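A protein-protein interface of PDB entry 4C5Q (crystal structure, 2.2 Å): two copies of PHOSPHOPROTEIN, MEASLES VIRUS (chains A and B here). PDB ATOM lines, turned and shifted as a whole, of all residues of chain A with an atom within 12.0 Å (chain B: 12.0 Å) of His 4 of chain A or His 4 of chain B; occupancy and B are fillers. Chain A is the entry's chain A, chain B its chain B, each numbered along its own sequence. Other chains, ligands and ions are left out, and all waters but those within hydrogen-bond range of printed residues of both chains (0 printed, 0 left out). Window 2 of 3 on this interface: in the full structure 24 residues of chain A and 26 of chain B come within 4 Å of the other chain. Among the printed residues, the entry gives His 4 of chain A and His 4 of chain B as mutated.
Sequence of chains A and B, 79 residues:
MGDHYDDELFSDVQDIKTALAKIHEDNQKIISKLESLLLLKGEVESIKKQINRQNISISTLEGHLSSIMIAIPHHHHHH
Of chain B, only His 4 comes within 4 Å of His 4 of chain A. His 4 of chain B touches two residues of chain A. Of chain B, only His 4 (3.3 Å) and Tyr 5 (3.7 Å) come within 4 Å of Asp 6 of chain A. No residue of chain A comes within 4 Å of Asp 6 of chain B. Printed residues of chain A within 4 Å of Leu 9 of chain B: Leu 9. Of the printed residues of chain B, Leu 9 of chain A touches Tyr 5 (3.4 Å) and Leu 9 (3.9 Å). Glu 8 of chain B touches none of the printed residues of chain A. Asp 7 of chain B touches none of the printed residues of chain A. The nearest residue of chain B that does not touch His 4 of chain A is Tyr 5 of chain B (5.8 Å). The nearest printed residue of chain B that does not touch Leu 9 of chain A is Val 13 of chain B (4.1 Å).
His 4 of chain A touches its own counterpart, His 4 of chain B. Asp 6 of chain A touches His 4 of chain B, but with the chains exchanged His 4 of chain A does not touch Asp 6 of chain B (8.1 Å). Asp 6 of chain A touches Tyr 5 of chain B, but with the chains exchanged Tyr 5 of chain A does not touch Asp 6 of chain B (9.3 Å). Leu 9 of chain A touches Tyr 5 of chain B, but with the chains exchanged Tyr 5 of chain A does not touch Leu 9 of chain B (7.9 Å). Of the 8 pairs that touch across the chains among the printed residues, 2 have their exchanged pair printed and touching as well.
ND1 of His 4 of chain B lies within hydrogen-bond range of OD2 of Asp 6 of chain A (3.3 Å). The side-chain carboxylate (OD2) of Asp 12 of chain A sits at hydrogen-bond distance from the side-chain hydroxyl (OH) of Tyr 5 of chain B, 2.6 Å away.
Among the printed residues, pairs that only touch across the chains: His 4 of chain A with His 4 of chain B (3.8 Å), Asp 6 of chain A with Tyr 5 of chain B (3.7 Å), Glu 8 of chain A with Tyr 5 of chain B (3.8 Å), Leu 9 of chain A with Tyr 5 of chain B (3.4 Å), Leu 9 of chain A with Leu 9 of chain B (3.9 Å) and Asp 12 of chain A with Val 13 of chain B (3.8 Å).
OD1 of Asp 6 of chain A sits at hydrogen-bond distance from N of Glu 8 of chain A, 2.8 Å away. OD1 of Asp 6 of chain A sits at hydrogen-bond distance from N of Leu 9 of chain A (3.1 Å). The side-chain carboxylate (OD1) of Asp 6 of chain B is in hydrogen-bond range of the backbone NH (N) of Leu 9 of chain B (3.1 Å).
Of the 10 printed residues of chain B, 4 touch a printed residue of chain A. Printed residues of chain B that touch a printed residue of chain A: His 4, Tyr 5, Leu 9 and Val 13. Among the printed residues, 8 pairs touch across the chains. Among the printed residues, no Asp or Glu carboxylate lies within 4 Å of a Lys or Arg side-chain nitrogen of the other chain.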
ATOM      1  N   HIS A   4     -14.250 -15.818  36.464  1.00  0.00           N
ATOM      2  CA  HIS A   4     -13.176 -16.624  37.035  1.00  0.00           C
ATOM      3  C   HIS A   4     -12.693 -17.666  36.032  1.00  0.00           C
ATOM      4  O   HIS A   4     -12.820 -17.480  34.820  1.00  0.00           O
ATOM      5  CB  HIS A   4     -13.664 -17.322  38.304  1.00  0.00           C
ATOM      6  CG  HIS A   4     -14.799 -18.272  38.069  1.00  0.00           C
ATOM      7  ND1 HIS A   4     -16.061 -17.853  37.708  1.00  0.00           N
ATOM      8  CD2 HIS A   4     -14.857 -19.622  38.141  1.00  0.00           C
ATOM      9  CE1 HIS A   4     -16.849 -18.904  37.567  1.00  0.00           C
ATOM     10  NE2 HIS A   4     -16.143 -19.991  37.828  1.00  0.00           N
ATOM     11  N   TYR A   5     -12.136 -18.757  36.550  1.00  0.00           N
ATOM     12  CA  TYR A   5     -11.746 -19.903  35.738  1.00  0.00           C
ATOM     13  C   TYR A   5     -12.761 -21.015  35.990  1.00  0.00           C
ATOM     14  O   TYR A   5     -12.607 -21.818  36.911  1.00  0.00           O
ATOM     15  CB  TYR A   5     -10.338 -20.355  36.129  1.00  0.00           C
ATOM     16  CG  TYR A   5      -9.619 -21.212  35.108  1.00  0.00           C
ATOM     17  CD1 TYR A   5     -10.291 -21.776  34.041  1.00  0.00           C
ATOM     18  CD2 TYR A   5      -8.259 -21.453  35.224  1.00  0.00           C
ATOM     19  CE1 TYR A   5      -9.622 -22.564  33.110  1.00  0.00           C
ATOM     20  CE2 TYR A   5      -7.589 -22.236  34.316  1.00  0.00           C
ATOM     21  CZ  TYR A   5      -8.269 -22.791  33.258  1.00  0.00           C
ATOM     22  OH  TYR A   5      -7.575 -23.570  32.346  1.00  0.00           O
ATOM     23  N   ASP A   6     -13.807 -21.044  35.176  1.00  0.00           N
ATOM     24  CA  ASP A   6     -14.902 -21.985  35.362  1.00  0.00           C
ATOM     25  C   ASP A   6     -14.459 -23.446  35.311  1.00  0.00           C
ATOM     26  O   ASP A   6     -13.650 -23.830  34.459  1.00  0.00           O
ATOM     27  CB  ASP A   6     -15.971 -21.735  34.308  1.00  0.00           C
ATOM     28  CG  ASP A   6     -17.030 -22.791  34.312  1.00  0.00           C
ATOM     29  OD1 ASP A   6     -16.812 -23.850  33.682  1.00  0.00           O
ATOM     30  OD2 ASP A   6     -18.071 -22.570  34.959  1.00  0.00           O
ATOM     31  N   ASP A   7     -15.011 -24.258  36.209  1.00  0.00           N
ATOM     32  CA  ASP A   7     -14.616 -25.662  36.349  1.00  0.00           C
ATOM     33  C   ASP A   7     -14.674 -26.508  35.071  1.00  0.00           C
ATOM     34  O   ASP A   7     -13.800 -27.348  34.837  1.00  0.00           O
ATOM     35  CB  ASP A   7     -15.459 -26.338  37.430  1.00  0.00           C
ATOM     36  CG  ASP A   7     -15.139 -25.837  38.825  1.00  0.00           C
ATOM     37  OD1 ASP A   7     -14.002 -25.376  39.060  1.00  0.00           O
ATOM     38  OD2 ASP A   7     -16.033 -25.917  39.687  1.00  0.00           O
ATOM     39  N   GLU A   8     -15.710 -26.319  34.262  1.00  0.00           N
ATOM     40  CA  GLU A   8     -15.829 -27.107  33.046  1.00  0.00           C
ATOM     41  C   GLU A   8     -14.890 -26.594  31.961  1.00  0.00           C
ATOM     42  O   GLU A   8     -14.322 -27.379  31.206  1.00  0.00           O
ATOM     43  CB  GLU A   8     -17.270 -27.157  32.549  1.00  0.00           C
ATOM     44  CG  GLU A   8     -17.882 -28.555  32.668  1.00  0.00           C
ATOM     45  CD  GLU A   8     -16.929 -29.668  32.209  1.00  0.00           C
ATOM     46  OE1 GLU A   8     -16.411 -29.600  31.069  1.00  0.00           O
ATOM     47  OE2 GLU A   8     -16.694 -30.613  32.998  1.00  0.00           O
ATOM     48  N   LEU A   9     -14.721 -25.277  31.898  1.00  0.00           N
ATOM     49  CA  LEU A   9     -13.695 -24.703  31.037  1.00  0.00           C
ATOM     50  C   LEU A   9     -12.332 -25.235  31.446  1.00  0.00           C
ATOM     51  O   LEU A   9     -11.549 -25.672  30.598  1.00  0.00           O
ATOM     52  CB  LEU A   9     -13.703 -23.180  31.101  1.00  0.00           C
ATOM     53  CG  LEU A   9     -12.511 -22.552  30.380  1.00  0.00           C
ATOM     54  CD1 LEU A   9     -12.507 -22.929  28.904  1.00  0.00           C
ATOM     55  CD2 LEU A   9     -12.489 -21.057  30.567  1.00  0.00           C
ATOM     56  N   PHE A  10     -12.052 -25.198  32.744  1.00  0.00           N
ATOM     57  CA  PHE A  10     -10.829 -25.786  33.261  1.00  0.00           C
ATOM     58  C   PHE A  10     -10.659 -27.218  32.766  1.00  0.00           C
ATOM     59  O   PHE A  10      -9.583 -27.608  32.310  1.00  0.00           O
ATOM     60  CB  PHE A  10     -10.807 -25.761  34.784  1.00  0.00           C
ATOM     61  CG  PHE A  10      -9.681 -26.558  35.370  1.00  0.00           C
ATOM     62  CD1 PHE A  10      -8.440 -25.977  35.571  1.00  0.00           C
ATOM     63  CD2 PHE A  10      -9.853 -27.898  35.687  1.00  0.00           C
ATOM     64  CE1 PHE A  10      -7.392 -26.719  36.083  1.00  0.00           C
ATOM     65  CE2 PHE A  10      -8.814 -28.638  36.191  1.00  0.00           C
ATOM     66  CZ  PHE A  10      -7.580 -28.047  36.392  1.00  0.00           C
ATOM     67  N   SER A  11     -11.727 -27.998  32.860  1.00  0.00           N
ATOM     68  CA  SER A  11     -11.675 -29.397  32.473  1.00  0.00           C
ATOM     69  C   SER A  11     -11.356 -29.523  30.992  1.00  0.00           C
ATOM     70  O   SER A  11     -10.523 -30.337  30.593  1.00  0.00           O
ATOM     71  CB  SER A  11     -13.008 -30.068  32.782  1.00  0.00           C
ATOM     72  OG  SER A  11     -13.014 -31.396  32.306  1.00  0.00           O
ATOM     73  N   ASP A  12     -12.031 -28.708  30.183  1.00  0.00           N
ATOM     74  CA  ASP A  12     -11.781 -28.652  28.754  1.00  0.00           C
ATOM     75  C   ASP A  12     -10.330 -28.293  28.440  1.00  0.00           C
ATOM     76  O   ASP A  12      -9.714 -28.878  27.540  1.00  0.00           O
ATOM     77  CB  ASP A  12     -12.701 -27.622  28.099  1.00  0.00           C
ATOM     78  CG  ASP A  12     -14.136 -28.071  28.063  1.00  0.00           C
ATOM     79  OD1 ASP A  12     -14.378 -29.282  28.242  1.00  0.00           O
ATOM     80  OD2 ASP A  12     -15.021 -27.210  27.848  1.00  0.00           O
ATOM     81  N   VAL A  13      -9.793 -27.319  29.161  1.00  0.00           N
ATOM     82  CA  VAL A  13      -8.399 -26.933  28.960  1.00  0.00           C
ATOM     83  C   VAL A  13      -7.448 -28.098  29.243  1.00  0.00           C
ATOM     84  O   VAL A  13      -6.507 -28.328  28.473  1.00  0.00           O
ATOM     85  CB  VAL A  13      -8.027 -25.708  29.789  1.00  0.00           C
ATOM     86  CG1 VAL A  13      -6.530 -25.474  29.767  1.00  0.00           C
ATOM     87  CG2 VAL A  13      -8.769 -24.483  29.266  1.00  0.00           C
ATOM     88  N   HIS B   4     -19.684 -17.047  33.267  1.00  0.00           N
ATOM     89  CA  HIS B   4     -18.665 -17.956  33.777  1.00  0.00           C
ATOM     90  C   HIS B   4     -17.870 -18.564  32.624  1.00  0.00           C
ATOM     91  O   HIS B   4     -16.756 -18.131  32.323  1.00  0.00           O
ATOM     92  CB  HIS B   4     -19.307 -19.048  34.641  1.00  0.00           C
ATOM     93  CG  HIS B   4     -20.513 -19.689  34.017  1.00  0.00           C
ATOM     94  ND1 HIS B   4     -20.463 -20.919  33.392  1.00  0.00           N
ATOM     95  CD2 HIS B   4     -21.795 -19.270  33.917  1.00  0.00           C
ATOM     96  CE1 HIS B   4     -21.663 -21.227  32.934  1.00  0.00           C
ATOM     97  NE2 HIS B   4     -22.491 -20.243  33.242  1.00  0.00           N
ATOM     98  N   TYR B   5     -18.456 -19.577  32.001  1.00  0.00           N
ATOM     99  CA  TYR B   5     -17.940 -20.185  30.795  1.00  0.00           C
ATOM    100  C   TYR B   5     -18.848 -19.650  29.694  1.00  0.00           C
ATOM    101  O   TYR B   5     -19.912 -20.206  29.437  1.00  0.00           O
ATOM    102  CB  TYR B   5     -18.058 -21.707  30.909  1.00  0.00           C
ATOM    103  CG  TYR B   5     -17.277 -22.511  29.885  1.00  0.00           C
ATOM    104  CD1 TYR B   5     -16.663 -21.901  28.804  1.00  0.00           C
ATOM    105  CD2 TYR B   5     -17.164 -23.884  30.009  1.00  0.00           C
ATOM    106  CE1 TYR B   5     -15.951 -22.644  27.872  1.00  0.00           C
ATOM    107  CE2 TYR B   5     -16.473 -24.633  29.086  1.00  0.00           C
ATOM    108  CZ  TYR B   5     -15.865 -24.011  28.021  1.00  0.00           C
ATOM    109  OH  TYR B   5     -15.167 -24.769  27.110  1.00  0.00           O
ATOM    110  N   ASP B   6     -18.433 -18.553  29.072  1.00  0.00           N
ATOM    111  CA  ASP B   6     -19.258 -17.848  28.093  1.00  0.00           C
ATOM    112  C   ASP B   6     -19.627 -18.733  26.904  1.00  0.00           C
ATOM    113  O   ASP B   6     -18.797 -19.504  26.418  1.00  0.00           O
ATOM    114  CB  ASP B   6     -18.537 -16.580  27.625  1.00  0.00           C
ATOM    115  CG  ASP B   6     -19.188 -15.951  26.416  1.00  0.00           C
ATOM    116  OD1 ASP B   6     -18.922 -16.416  25.288  1.00  0.00           O
ATOM    117  OD2 ASP B   6     -19.962 -14.989  26.588  1.00  0.00           O
ATOM    118  N   ASP B   7     -20.871 -18.607  26.446  1.00  0.00           N
ATOM    119  CA  ASP B   7     -21.404 -19.432  25.368  1.00  0.00           C
ATOM    120  C   ASP B   7     -20.523 -19.477  24.120  1.00  0.00           C
ATOM    121  O   ASP B   7     -20.334 -20.543  23.523  1.00  0.00           O
ATOM    122  CB  ASP B   7     -22.806 -18.953  24.966  1.00  0.00           C
ATOM    123  CG  ASP B   7     -23.879 -19.315  25.988  1.00  0.00           C
ATOM    124  OD1 ASP B   7     -23.571 -19.949  27.018  1.00  0.00           O
ATOM    125  OD2 ASP B   7     -25.049 -18.970  25.738  1.00  0.00           O
ATOM    126  N   GLU B   8     -20.001 -18.328  23.703  1.00  0.00           N
ATOM    127  CA  GLU B   8     -19.219 -18.309  22.473  1.00  0.00           C
ATOM    128  C   GLU B   8     -17.803 -18.819  22.685  1.00  0.00           C
ATOM    129  O   GLU B   8     -17.244 -19.491  21.814  1.00  0.00           O
ATOM    130  CB  GLU B   8     -19.219 -16.935  21.808  1.00  0.00           C
ATOM    131  CG  GLU B   8     -19.977 -16.943  20.480  1.00  0.00           C
ATOM    132  CD  GLU B   8     -19.635 -18.159  19.606  1.00  0.00           C
ATOM    133  OE1 GLU B   8     -18.432 -18.422  19.359  1.00  0.00           O
ATOM    134  OE2 GLU B   8     -20.577 -18.860  19.167  1.00  0.00           O
ATOM    135  N   LEU B   9     -17.231 -18.524  23.845  1.00  0.00           N
ATOM    136  CA  LEU B   9     -15.960 -19.146  24.201  1.00  0.00           C
ATOM    137  C   LEU B   9     -16.154 -20.664  24.235  1.00  0.00           C
ATOM    138  O   LEU B   9     -15.301 -21.414  23.759  1.00  0.00           O
ATOM    139  CB  LEU B   9     -15.436 -18.631  25.540  1.00  0.00           C
ATOM    140  CG  LEU B   9     -14.282 -19.444  26.130  1.00  0.00           C
ATOM    141  CD1 LEU B   9     -13.001 -19.341  25.264  1.00  0.00           C
ATOM    142  CD2 LEU B   9     -14.017 -19.095  27.599  1.00  0.00           C
ATOM    143  N   PHE B  10     -17.295 -21.100  24.764  1.00  0.00           N
ATOM    144  CA  PHE B  10     -17.631 -22.511  24.795  1.00  0.00           C
ATOM    145  C   PHE B  10     -17.691 -23.097  23.387  1.00  0.00           C
ATOM    146  O   PHE B  10     -17.212 -24.205  23.148  1.00  0.00           O
ATOM    147  CB  PHE B  10     -18.959 -22.721  25.518  1.00  0.00           C
ATOM    148  CG  PHE B  10     -19.533 -24.088  25.328  1.00  0.00           C
ATOM    149  CD1 PHE B  10     -19.150 -25.133  26.150  1.00  0.00           C
ATOM    150  CD2 PHE B  10     -20.454 -24.332  24.319  1.00  0.00           C
ATOM    151  CE1 PHE B  10     -19.668 -26.397  25.961  1.00  0.00           C
ATOM    152  CE2 PHE B  10     -20.964 -25.585  24.127  1.00  0.00           C
ATOM    153  CZ  PHE B  10     -20.576 -26.620  24.950  1.00  0.00           C
ATOM    154  N   SER B  11     -18.288 -22.357  22.458  1.00  0.00           N
ATOM    155  CA  SER B  11     -18.397 -22.833  21.091  1.00  0.00           C
ATOM    156  C   SER B  11     -17.005 -22.954  20.483  1.00  0.00           C
ATOM    157  O   SER B  11     -16.667 -23.966  19.867  1.00  0.00           O
ATOM    158  CB  SER B  11     -19.276 -21.899  20.262  1.00  0.00           C
ATOM    159  OG  SER B  11     -19.149 -22.192  18.882  1.00  0.00           O
ATOM    160  N   VAL B  13     -14.278 -23.445  22.100  1.00  0.00           N
ATOM    161  CA  VAL B  13     -13.529 -24.545  22.699  1.00  0.00           C
ATOM    162  C   VAL B  13     -13.892 -25.888  22.032  1.00  0.00           C
ATOM    163  O   VAL B  13     -13.015 -26.720  21.789  1.00  0.00           O
ATOM    164  CB  VAL B  13     -13.668 -24.578  24.232  1.00  0.00           C
ATOM    165  CG1 VAL B  13     -13.034 -25.824  24.802  1.00  0.00           C
ATOM    166  CG2 VAL B  13     -13.014 -23.343  24.848  1.00  0.00           C
ATOM    167  N   GLN B  14     -15.168 -26.065  21.680  1.00  0.00           N
ATOM    168  CA  GLN B  14     -15.632 -27.304  21.050  1.00  0.00           C
ATOM    169  C   GLN B  14     -15.039 -27.491  19.670  1.00  0.00           C
ATOM    170  O   GLN B  14     -14.739 -28.616  19.258  1.00  0.00           O
ATOM    171  CB  GLN B  14     -17.158 -27.330  20.929  1.00  0.00           C
ATOM    172  CG  GLN B  14     -17.882 -27.247  22.258  1.00  0.00           C
ATOM    173  CD  GLN B  14     -17.277 -28.160  23.306  1.00  0.00           C
ATOM    174  OE1 GLN B  14     -17.055 -27.750  24.437  1.00  0.00           O
ATOM    175  NE2 GLN B  14     -17.015 -29.409  22.933  1.00  0.00           N
